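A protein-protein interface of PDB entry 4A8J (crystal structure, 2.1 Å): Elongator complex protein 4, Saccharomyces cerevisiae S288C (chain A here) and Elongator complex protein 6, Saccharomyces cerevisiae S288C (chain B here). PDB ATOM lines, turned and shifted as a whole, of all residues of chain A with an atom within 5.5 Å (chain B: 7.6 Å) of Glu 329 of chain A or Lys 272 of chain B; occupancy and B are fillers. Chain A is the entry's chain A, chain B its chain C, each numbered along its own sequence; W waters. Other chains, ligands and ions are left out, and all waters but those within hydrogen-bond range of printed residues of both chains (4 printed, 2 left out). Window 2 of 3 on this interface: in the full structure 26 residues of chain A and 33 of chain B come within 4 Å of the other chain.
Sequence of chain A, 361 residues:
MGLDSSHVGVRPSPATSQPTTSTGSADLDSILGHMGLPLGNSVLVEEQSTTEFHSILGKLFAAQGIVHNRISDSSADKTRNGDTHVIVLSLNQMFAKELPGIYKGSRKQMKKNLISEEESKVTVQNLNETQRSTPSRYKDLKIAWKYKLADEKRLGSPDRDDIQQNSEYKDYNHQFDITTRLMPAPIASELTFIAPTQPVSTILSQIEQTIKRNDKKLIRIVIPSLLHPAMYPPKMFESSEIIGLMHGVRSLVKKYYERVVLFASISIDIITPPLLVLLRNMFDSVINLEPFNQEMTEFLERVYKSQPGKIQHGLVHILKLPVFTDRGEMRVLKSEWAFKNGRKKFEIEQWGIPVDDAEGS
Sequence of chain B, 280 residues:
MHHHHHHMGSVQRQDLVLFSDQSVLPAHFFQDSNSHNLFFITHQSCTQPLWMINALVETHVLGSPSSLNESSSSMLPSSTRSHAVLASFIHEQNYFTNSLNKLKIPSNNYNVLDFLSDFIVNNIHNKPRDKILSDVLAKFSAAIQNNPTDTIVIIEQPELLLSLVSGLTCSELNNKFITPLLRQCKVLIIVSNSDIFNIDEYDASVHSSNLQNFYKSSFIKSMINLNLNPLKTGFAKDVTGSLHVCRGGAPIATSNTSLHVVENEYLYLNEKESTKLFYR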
ATOM      1  N   PHE A 324      -6.153 -23.681   8.436  1.00  0.00           N
ATOM      2  CA  PHE A 324      -6.256 -24.756   9.423  1.00  0.00           C
ATOM      3  C   PHE A 324      -5.033 -24.855  10.350  1.00  0.00           C
ATOM      4  O   PHE A 324      -5.154 -24.884  11.590  1.00  0.00           O
ATOM      5  CB  PHE A 324      -6.497 -26.089   8.711  1.00  0.00           C
ATOM      6  CG  PHE A 324      -7.662 -26.051   7.747  1.00  0.00           C
ATOM      7  CD1 PHE A 324      -8.903 -25.596   8.161  1.00  0.00           C
ATOM      8  CD2 PHE A 324      -7.498 -26.437   6.421  1.00  0.00           C
ATOM      9  CE1 PHE A 324      -9.991 -25.548   7.276  1.00  0.00           C
ATOM     10  CE2 PHE A 324      -8.582 -26.396   5.521  1.00  0.00           C
ATOM     11  CZ  PHE A 324      -9.828 -25.944   5.963  1.00  0.00           C
ATOM     12  N   THR A 325      -3.852 -24.924   9.750  1.00  0.00           N
ATOM     13  CA  THR A 325      -2.631 -25.024  10.546  1.00  0.00           C
ATOM     14  C   THR A 325      -2.448 -23.813  11.469  1.00  0.00           C
ATOM     15  O   THR A 325      -2.204 -23.980  12.663  1.00  0.00           O
ATOM     16  CB  THR A 325      -1.393 -25.244   9.661  1.00  0.00           C
ATOM     17  OG1 THR A 325      -1.538 -26.487   8.964  1.00  0.00           O
ATOM     18  CG2 THR A 325      -0.107 -25.283  10.509  1.00  0.00           C
ATOM     19  N   ARG A 327      -4.468 -21.819  12.889  1.00  0.00           N
ATOM     20  CA  ARG A 327      -5.343 -21.697  14.044  1.00  0.00           C
ATOM     21  C   ARG A 327      -5.134 -22.813  15.076  1.00  0.00           C
ATOM     22  O   ARG A 327      -5.648 -22.733  16.202  1.00  0.00           O
ATOM     23  CB  ARG A 327      -6.810 -21.529  13.642  1.00  0.00           C
ATOM     24  CG  ARG A 327      -7.406 -22.679  12.906  1.00  0.00           C
ATOM     25  CD  ARG A 327      -8.732 -22.256  12.320  1.00  0.00           C
ATOM     26  NE  ARG A 327      -9.509 -23.412  11.897  1.00  0.00           N
ATOM     27  CZ  ARG A 327     -10.611 -23.353  11.155  1.00  0.00           C
ATOM     28  NH1 ARG A 327     -11.082 -22.182  10.735  1.00  0.00           N
ATOM     29  NH2 ARG A 327     -11.241 -24.478  10.840  1.00  0.00           N
ATOM     30  N   GLY A 328      -4.355 -23.832  14.706  1.00  0.00           N
ATOM     31  CA  GLY A 328      -3.889 -24.809  15.678  1.00  0.00           C
ATOM     32  C   GLY A 328      -4.130 -26.273  15.387  1.00  0.00           C
ATOM     33  O   GLY A 328      -3.853 -27.117  16.238  1.00  0.00           O
ATOM     34  N   GLU A 329      -4.644 -26.584  14.203  1.00  0.00           N
ATOM     35  CA  GLU A 329      -4.905 -27.966  13.836  1.00  0.00           C
ATOM     36  C   GLU A 329      -3.620 -28.669  13.381  1.00  0.00           C
ATOM     37  O   GLU A 329      -2.716 -28.048  12.797  1.00  0.00           O
ATOM     38  CB  GLU A 329      -5.986 -28.057  12.739  1.00  0.00           C
ATOM     39  CG  GLU A 329      -7.233 -27.248  13.027  1.00  0.00           C
ATOM     40  CD  GLU A 329      -8.405 -27.577  12.107  1.00  0.00           C
ATOM     41  OE1 GLU A 329      -8.277 -28.445  11.229  1.00  0.00           O
ATOM     42  OE2 GLU A 329      -9.479 -26.962  12.276  1.00  0.00           O
ATOM     43  N   MET A 330      -3.550 -29.968  13.671  1.00  0.00           N
ATOM     44  CA  MET A 330      -2.451 -30.823  13.251  1.00  0.00           C
ATOM     45  C   MET A 330      -2.871 -31.455  11.930  1.00  0.00           C
ATOM     46  O   MET A 330      -3.696 -32.383  11.910  1.00  0.00           O
ATOM     47  CB  MET A 330      -2.197 -31.906  14.311  1.00  0.00           C
ATOM     48  CG  MET A 330      -0.741 -32.246  14.524  1.00  0.00           C
ATOM     49  SD  MET A 330       0.000 -33.159  12.950  1.00  0.00           S
ATOM     50  CE  MET A 330      -1.156 -34.771  12.944  1.00  0.00           C
ATOM     51  N   ARG A 331      -2.323 -30.942  10.829  1.00  0.00           N
ATOM     52  CA  ARG A 331      -2.763 -31.363   9.504  1.00  0.00           C
ATOM     53  C   ARG A 331      -1.706 -32.163   8.768  1.00  0.00           C
ATOM     54  O   ARG A 331      -1.888 -32.497   7.608  1.00  0.00           O
ATOM     55  CB  ARG A 331      -3.183 -30.161   8.659  1.00  0.00           C
ATOM     56  CG  ARG A 331      -4.358 -29.349   9.252  1.00  0.00           C
ATOM     57  CD  ARG A 331      -5.607 -30.208   9.549  1.00  0.00           C
ATOM     58  NE  ARG A 331      -6.251 -30.685   8.327  1.00  0.00           N
ATOM     59  CZ  ARG A 331      -7.423 -30.247   7.863  1.00  0.00           C
ATOM     60  NH1 ARG A 331      -8.106 -29.310   8.514  1.00  0.00           N
ATOM     61  NH2 ARG A 331      -7.909 -30.746   6.729  1.00  0.00           N
ATOM     62  N   SER B  45       5.583 -26.280  14.614  1.00  0.00           N
ATOM     63  CA  SER B  45       4.771 -25.536  13.653  1.00  0.00           C
ATOM     64  C   SER B  45       3.525 -26.295  13.208  1.00  0.00           C
ATOM     65  O   SER B  45       2.623 -25.701  12.606  1.00  0.00           O
ATOM     66  CB  SER B  45       5.603 -25.059  12.443  1.00  0.00           C
ATOM     67  OG  SER B  45       6.310 -26.122  11.840  1.00  0.00           O
ATOM     68  N   CYS B  46       3.462 -27.593  13.492  1.00  0.00           N
ATOM     69  CA  CYS B  46       2.214 -28.338  13.289  1.00  0.00           C
ATOM     70  C   CYS B  46       1.240 -28.259  14.477  1.00  0.00           C
ATOM     71  O   CYS B  46       0.096 -28.682  14.361  1.00  0.00           O
ATOM     72  CB  CYS B  46       2.504 -29.798  12.978  1.00  0.00           C
ATOM     73  SG  CYS B  46       3.407 -30.604  14.277  1.00  0.00           S
ATOM     74  N   THR B  47       1.693 -27.739  15.621  1.00  0.00           N
ATOM     75  CA  THR B  47       0.794 -27.482  16.756  1.00  0.00           C
ATOM     76  C   THR B  47       0.865 -26.020  17.183  1.00  0.00           C
ATOM     77  O   THR B  47       1.455 -25.682  18.221  1.00  0.00           O
ATOM     78  CB  THR B  47       1.115 -28.415  17.960  1.00  0.00           C
ATOM     79  OG1 THR B  47       2.499 -28.279  18.303  1.00  0.00           O
ATOM     80  CG2 THR B  47       0.860 -29.881  17.580  1.00  0.00           C
ATOM     81  N   GLN B  48       0.266 -25.153  16.376  1.00  0.00           N
ATOM     82  CA  GLN B  48       0.377 -23.706  16.579  1.00  0.00           C
ATOM     83  C   GLN B  48      -0.420 -23.183  17.798  1.00  0.00           C
ATOM     84  O   GLN B  48      -1.381 -23.818  18.229  1.00  0.00           O
ATOM     85  CB  GLN B  48      -0.074 -22.995  15.315  1.00  0.00           C
ATOM     86  CG  GLN B  48       0.748 -23.372  14.127  1.00  0.00           C
ATOM     87  CD  GLN B  48       1.837 -22.387  13.864  1.00  0.00           C
ATOM     88  OE1 GLN B  48       2.963 -22.768  13.542  1.00  0.00           O
ATOM     89  NE2 GLN B  48       1.511 -21.100  13.971  1.00  0.00           N
ATOM     90  N   TRP B  51      -4.755 -20.504  19.795  1.00  0.00           N
ATOM     91  CA  TRP B  51      -5.811 -20.691  20.790  1.00  0.00           C
ATOM     92  C   TRP B  51      -5.305 -20.446  22.212  1.00  0.00           C
ATOM     93  O   TRP B  51      -6.066 -20.031  23.082  1.00  0.00           O
ATOM     94  CB  TRP B  51      -6.441 -22.082  20.684  1.00  0.00           C
ATOM     95  CG  TRP B  51      -5.451 -23.197  20.846  1.00  0.00           C
ATOM     96  CD1 TRP B  51      -4.779 -23.842  19.855  1.00  0.00           C
ATOM     97  CD2 TRP B  51      -5.031 -23.809  22.093  1.00  0.00           C
ATOM     98  NE1 TRP B  51      -3.962 -24.817  20.403  1.00  0.00           N
ATOM     99  CE2 TRP B  51      -4.105 -24.813  21.744  1.00  0.00           C
ATOM    100  CE3 TRP B  51      -5.374 -23.606  23.430  1.00  0.00           C
ATOM    101  CZ2 TRP B  51      -3.507 -25.614  22.731  1.00  0.00           C
ATOM    102  CZ3 TRP B  51      -4.769 -24.399  24.388  1.00  0.00           C
ATOM    103  CH2 TRP B  51      -3.854 -25.394  24.035  1.00  0.00           C
ATOM    104  N   THR B 240      -5.095 -33.417  18.802  1.00  0.00           N
ATOM    105  CA  THR B 240      -4.171 -32.559  18.069  1.00  0.00           C
ATOM    106  C   THR B 240      -2.759 -32.773  18.602  1.00  0.00           C
ATOM    107  O   THR B 240      -1.832 -33.023  17.844  1.00  0.00           O
ATOM    108  CB  THR B 240      -4.562 -31.090  18.203  1.00  0.00           C
ATOM    109  OG1 THR B 240      -5.861 -30.902  17.657  1.00  0.00           O
ATOM    110  CG2 THR B 240      -3.605 -30.197  17.462  1.00  0.00           C
ATOM    111  N   TYR B 268      -4.991 -32.304  23.942  1.00  0.00           N
ATOM    112  CA  TYR B 268      -5.991 -31.342  23.530  1.00  0.00           C
ATOM    113  C   TYR B 268      -6.375 -31.643  22.105  1.00  0.00           C
ATOM    114  O   TYR B 268      -5.602 -32.240  21.352  1.00  0.00           O
ATOM    115  CB  TYR B 268      -5.506 -29.883  23.679  1.00  0.00           C
ATOM    116  CG  TYR B 268      -4.407 -29.462  22.689  1.00  0.00           C
ATOM    117  CD1 TYR B 268      -3.053 -29.633  22.990  1.00  0.00           C
ATOM    118  CD2 TYR B 268      -4.731 -28.865  21.482  1.00  0.00           C
ATOM    119  CE1 TYR B 268      -2.058 -29.237  22.086  1.00  0.00           C
ATOM    120  CE2 TYR B 268      -3.750 -28.468  20.582  1.00  0.00           C
ATOM    121  CZ  TYR B 268      -2.420 -28.656  20.884  1.00  0.00           C
ATOM    122  OH  TYR B 268      -1.462 -28.251  19.978  1.00  0.00           O
ATOM    123  N   LEU B 269      -7.595 -31.256  21.757  1.00  0.00           N
ATOM    124  CA  LEU B 269      -8.064 -31.336  20.387  1.00  0.00           C
ATOM    125  C   LEU B 269      -8.472 -29.935  19.978  1.00  0.00           C
ATOM    126  O   LEU B 269      -9.314 -29.310  20.620  1.00  0.00           O
ATOM    127  CB  LEU B 269      -9.272 -32.261  20.283  1.00  0.00           C
ATOM    128  CG  LEU B 269      -9.936 -32.210  18.908  1.00  0.00           C
ATOM    129  CD1 LEU B 269      -8.974 -32.763  17.840  1.00  0.00           C
ATOM    130  CD2 LEU B 269     -11.252 -32.994  18.919  1.00  0.00           C
ATOM    131  N   ASN B 270      -7.844 -29.426  18.930  1.00  0.00           N
ATOM    132  CA  ASN B 270      -8.255 -28.166  18.340  1.00  0.00           C
ATOM    133  C   ASN B 270      -8.882 -28.436  16.965  1.00  0.00           C
ATOM    134  O   ASN B 270      -8.266 -29.074  16.085  1.00  0.00           O
ATOM    135  CB  ASN B 270      -7.063 -27.208  18.191  1.00  0.00           C
ATOM    136  CG  ASN B 270      -7.447 -25.908  17.494  1.00  0.00           C
ATOM    137  OD1 ASN B 270      -7.407 -25.815  16.257  1.00  0.00           O
ATOM    138  ND2 ASN B 270      -7.856 -24.901  18.284  1.00  0.00           N
ATOM    139  N   GLU B 271     -10.112 -27.966  16.790  1.00  0.00           N
ATOM    140  CA  GLU B 271     -10.795 -28.032  15.489  1.00  0.00           C
ATOM    141  C   GLU B 271     -12.059 -27.170  15.448  1.00  0.00           C
ATOM    142  O   GLU B 271     -12.668 -26.901  16.480  1.00  0.00           O
ATOM    143  CB  GLU B 271     -11.094 -29.479  15.081  1.00  0.00           C
ATOM    144  CG  GLU B 271     -12.086 -30.234  15.939  1.00  0.00           C
ATOM    145  CD  GLU B 271     -12.450 -31.585  15.326  1.00  0.00           C
ATOM    146  OE1 GLU B 271     -11.942 -31.905  14.221  1.00  0.00           O
ATOM    147  OE2 GLU B 271     -13.241 -32.328  15.947  1.00  0.00           O
ATOM    148  N   LYS B 272     -12.440 -26.728  14.251  1.00  0.00           N
ATOM    149  CA  LYS B 272     -13.537 -25.771  14.085  1.00  0.00           C
ATOM    150  C   LYS B 272     -13.380 -24.578  15.023  1.00  0.00           C
ATOM    151  O   LYS B 272     -14.363 -24.114  15.600  1.00  0.00           O
ATOM    152  CB  LYS B 272     -14.897 -26.415  14.361  1.00  0.00           C
ATOM    153  CG  LYS B 272     -14.935 -27.925  14.258  1.00  0.00           C
ATOM    154  CD  LYS B 272     -15.229 -28.395  12.851  1.00  0.00           C
ATOM    155  N   GLU B 273     -12.151 -24.096  15.183  1.00  0.00           N
ATOM    156  CA  GLU B 273     -11.901 -22.891  15.969  1.00  0.00           C
ATOM    157  C   GLU B 273     -12.259 -23.083  17.431  1.00  0.00           C
ATOM    158  O   GLU B 273     -12.430 -22.104  18.149  1.00  0.00           O
ATOM    159  CB  GLU B 273     -12.700 -21.709  15.417  1.00  0.00           C
ATOM    160  CG  GLU B 273     -12.420 -21.391  13.954  1.00  0.00           C
ATOM    161  CD  GLU B 273     -13.346 -20.324  13.411  1.00  0.00           C
ATOM    162  OE1 GLU B 273     -14.563 -20.587  13.309  1.00  0.00           O
ATOM    163  OE2 GLU B 273     -12.853 -19.222  13.095  1.00  0.00           O
ATOM    164  N   SER B 274     -12.390 -24.330  17.870  1.00  0.00           N
ATOM    165  CA  SER B 274     -12.610 -24.588  19.294  1.00  0.00           C
ATOM    166  C   SER B 274     -11.620 -25.625  19.831  1.00  0.00           C
ATOM    167  O   SER B 274     -11.193 -26.536  19.100  1.00  0.00           O
ATOM    168  CB  SER B 274     -14.043 -25.045  19.558  1.00  0.00           C
ATOM    169  OG  SER B 274     -14.124 -26.457  19.498  1.00  0.00           O
ATOM    170  N   THR B 275     -11.271 -25.492  21.109  1.00  0.00           N
ATOM    171  CA  THR B 275     -10.239 -26.348  21.694  1.00  0.00           C
ATOM    172  C   THR B 275     -10.741 -27.012  22.953  1.00  0.00           C
ATOM    173  O   THR B 275     -11.449 -26.407  23.735  1.00  0.00           O
ATOM    174  CB  THR B 275      -8.953 -25.557  22.032  1.00  0.00           C
ATOM    175  OG1 THR B 275      -8.558 -24.781  20.901  1.00  0.00           O
ATOM    176  CG2 THR B 275      -7.794 -26.497  22.437  1.00  0.00           C
HETATM  177  O   HOH W   1     -10.422 -19.518  10.775  1.00  0.00           O
HETATM  178  O   HOH W   2      -2.288 -26.360  18.376  1.00  0.00           O
HETATM  179  O   HOH W   3     -11.499 -28.474  11.511  1.00  0.00           O
HETATM  180  O   HOH W   4      -5.908 -31.331  14.967  1.00  0.00           O
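Of the 7 printed residues of chain A, 5 touch a printed residue of chain B. Hydrophobic or aromatic side chains of chain A that line the printed part of chain B: Met 330. Hydrophobic or aromatic side chains of chain B that line the printed part of chain A: Trp 51. Along chain B the printed residues that touch a printed residue of chain A span positions 45 to 273. Among the printed residues, 14 pairs touch across the chains.
The backbone NH (N) of Glu 329 of chain A is in hydrogen-bond range of the backbone carbonyl oxygen (O) of Phe 324 of chain A (3.2 Å). The side-chain carboxylate of Glu 329 of chain A lies within salt-bridge range of the guanidinium group of Arg 327 of chain A (3.4 Å). OE1 of Glu 329 of chain A lies within salt-bridge range of NH1 of Arg 331 of chain A, at 2.9 Å. The side-chain hydroxyl (OG1) of Thr 240 of chain B is in hydrogen-bond range of the backbone NH (N) of Asn 270 of chain B. OG1 of Thr 275 of chain B lies within hydrogen-bond range of ND2 of Asn 270 of chain B (2.7 Å). The backbone carbonyl oxygen (O) of Glu 271 of chain B is in hydrogen-bond range of the side-chain hydroxyl (OG) of Ser 274 of chain B (3.4 Å).
Glu 329 of chain A touches just these residues of chain B: Cys 46, Asn 270, Glu 271 and Lys 272. Lys 272 of chain B touches one residue of chain A. Of chain B, only Gln 48 (3.7 Å), Thr 240 (3.3 Å) and Asn 270 (3.4 Å) come within 4 Å of Gly 328 of chain A. Of the printed residues of chain B, Met 330 of chain A touches Cys 46 (3.5 Å) and Thr 240 (3.6 Å). Printed residues of chain A within 4 Å of Cys 46 of chain B: Glu 329 and Met 330. Printed residues of chain A within 4 Å of Asn 270 of chain B: Arg 327 (3.5 Å), Gly 328 (3.4 Å) and Glu 329 (3.5 Å). Printed residues of chain A within 4 Å of Glu 271 of chain B: Glu 329. Of the printed residues of chain B, Arg 327 of chain A touches Trp 51 (3.9 Å), Asn 270 (3.5 Å) and Glu 273 (3.6 Å). Thr 275 of chain B touches none of the printed residues of chain A. Phe 324 of chain A touches none of the printed residues of chain B.
Water W2 lies within hydrogen-bond range of the side-chain hydroxyl of Tyr 268 of chain B (2.6 Å), the backbone carbonyl oxygen of Gln 48 of chain B (2.7 Å), the backbone carbonyl oxygen of Gly 328 of chain A (2.8 Å) and the indole nitrogen of Trp 51 of chain B (3.0 Å). Water W3 bridges OE2 of Glu 329 of chain A (2.6 Å) and N of Lys 272 of chain B (3.4 Å). Water W4 lies within hydrogen-bond range of the side-chain hydroxyl (OG1) of Thr 240 of chain B (2.7 Å), the backbone NH (N) of Met 330 of chain A (3.0 Å) and the backbone carbonyl oxygen (O) of Asn 270 of chain B (3.5 Å). Water W1 bridges the guanidinium group (NH1) of Arg 327 of chain A (2.7 Å) and the side-chain carboxylate (OE2) of Glu 273 of chain B (3.4 Å).
Ser 45 of chain B touches Thr 325 of chain A. CG of Gln 48 of chain B touches O of Thr 325 of chain A (3.4 Å). O of Arg 327 of chain A touches OD1 of Asn 270 of chain B, 3.5 Å away. CG of Glu 273 of chain B touches NH1 of Arg 327 of chain A, at 3.6 Å. Thr 240 of chain B touches Gly 328 of chain A. Gly 328 of chain A touches Asn 270 of chain B. OD1 of Asn 270 of chain B touches N of Glu 329 of chain A, at 3.5 Å. Glu 271 of chain B touches Glu 329 of chain A (CA to OE2, 3.6 Å). Met 330 of chain A touches Cys 46 of chain B. Thr 240 of chain B touches Met 330 of chain A (O to CG, 3.6 Å).
The backbone carbonyl oxygen of Cys 46 of chain B lies close to the backbone carbonyl oxygen of Glu 329 of chain A (3.3 Å).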
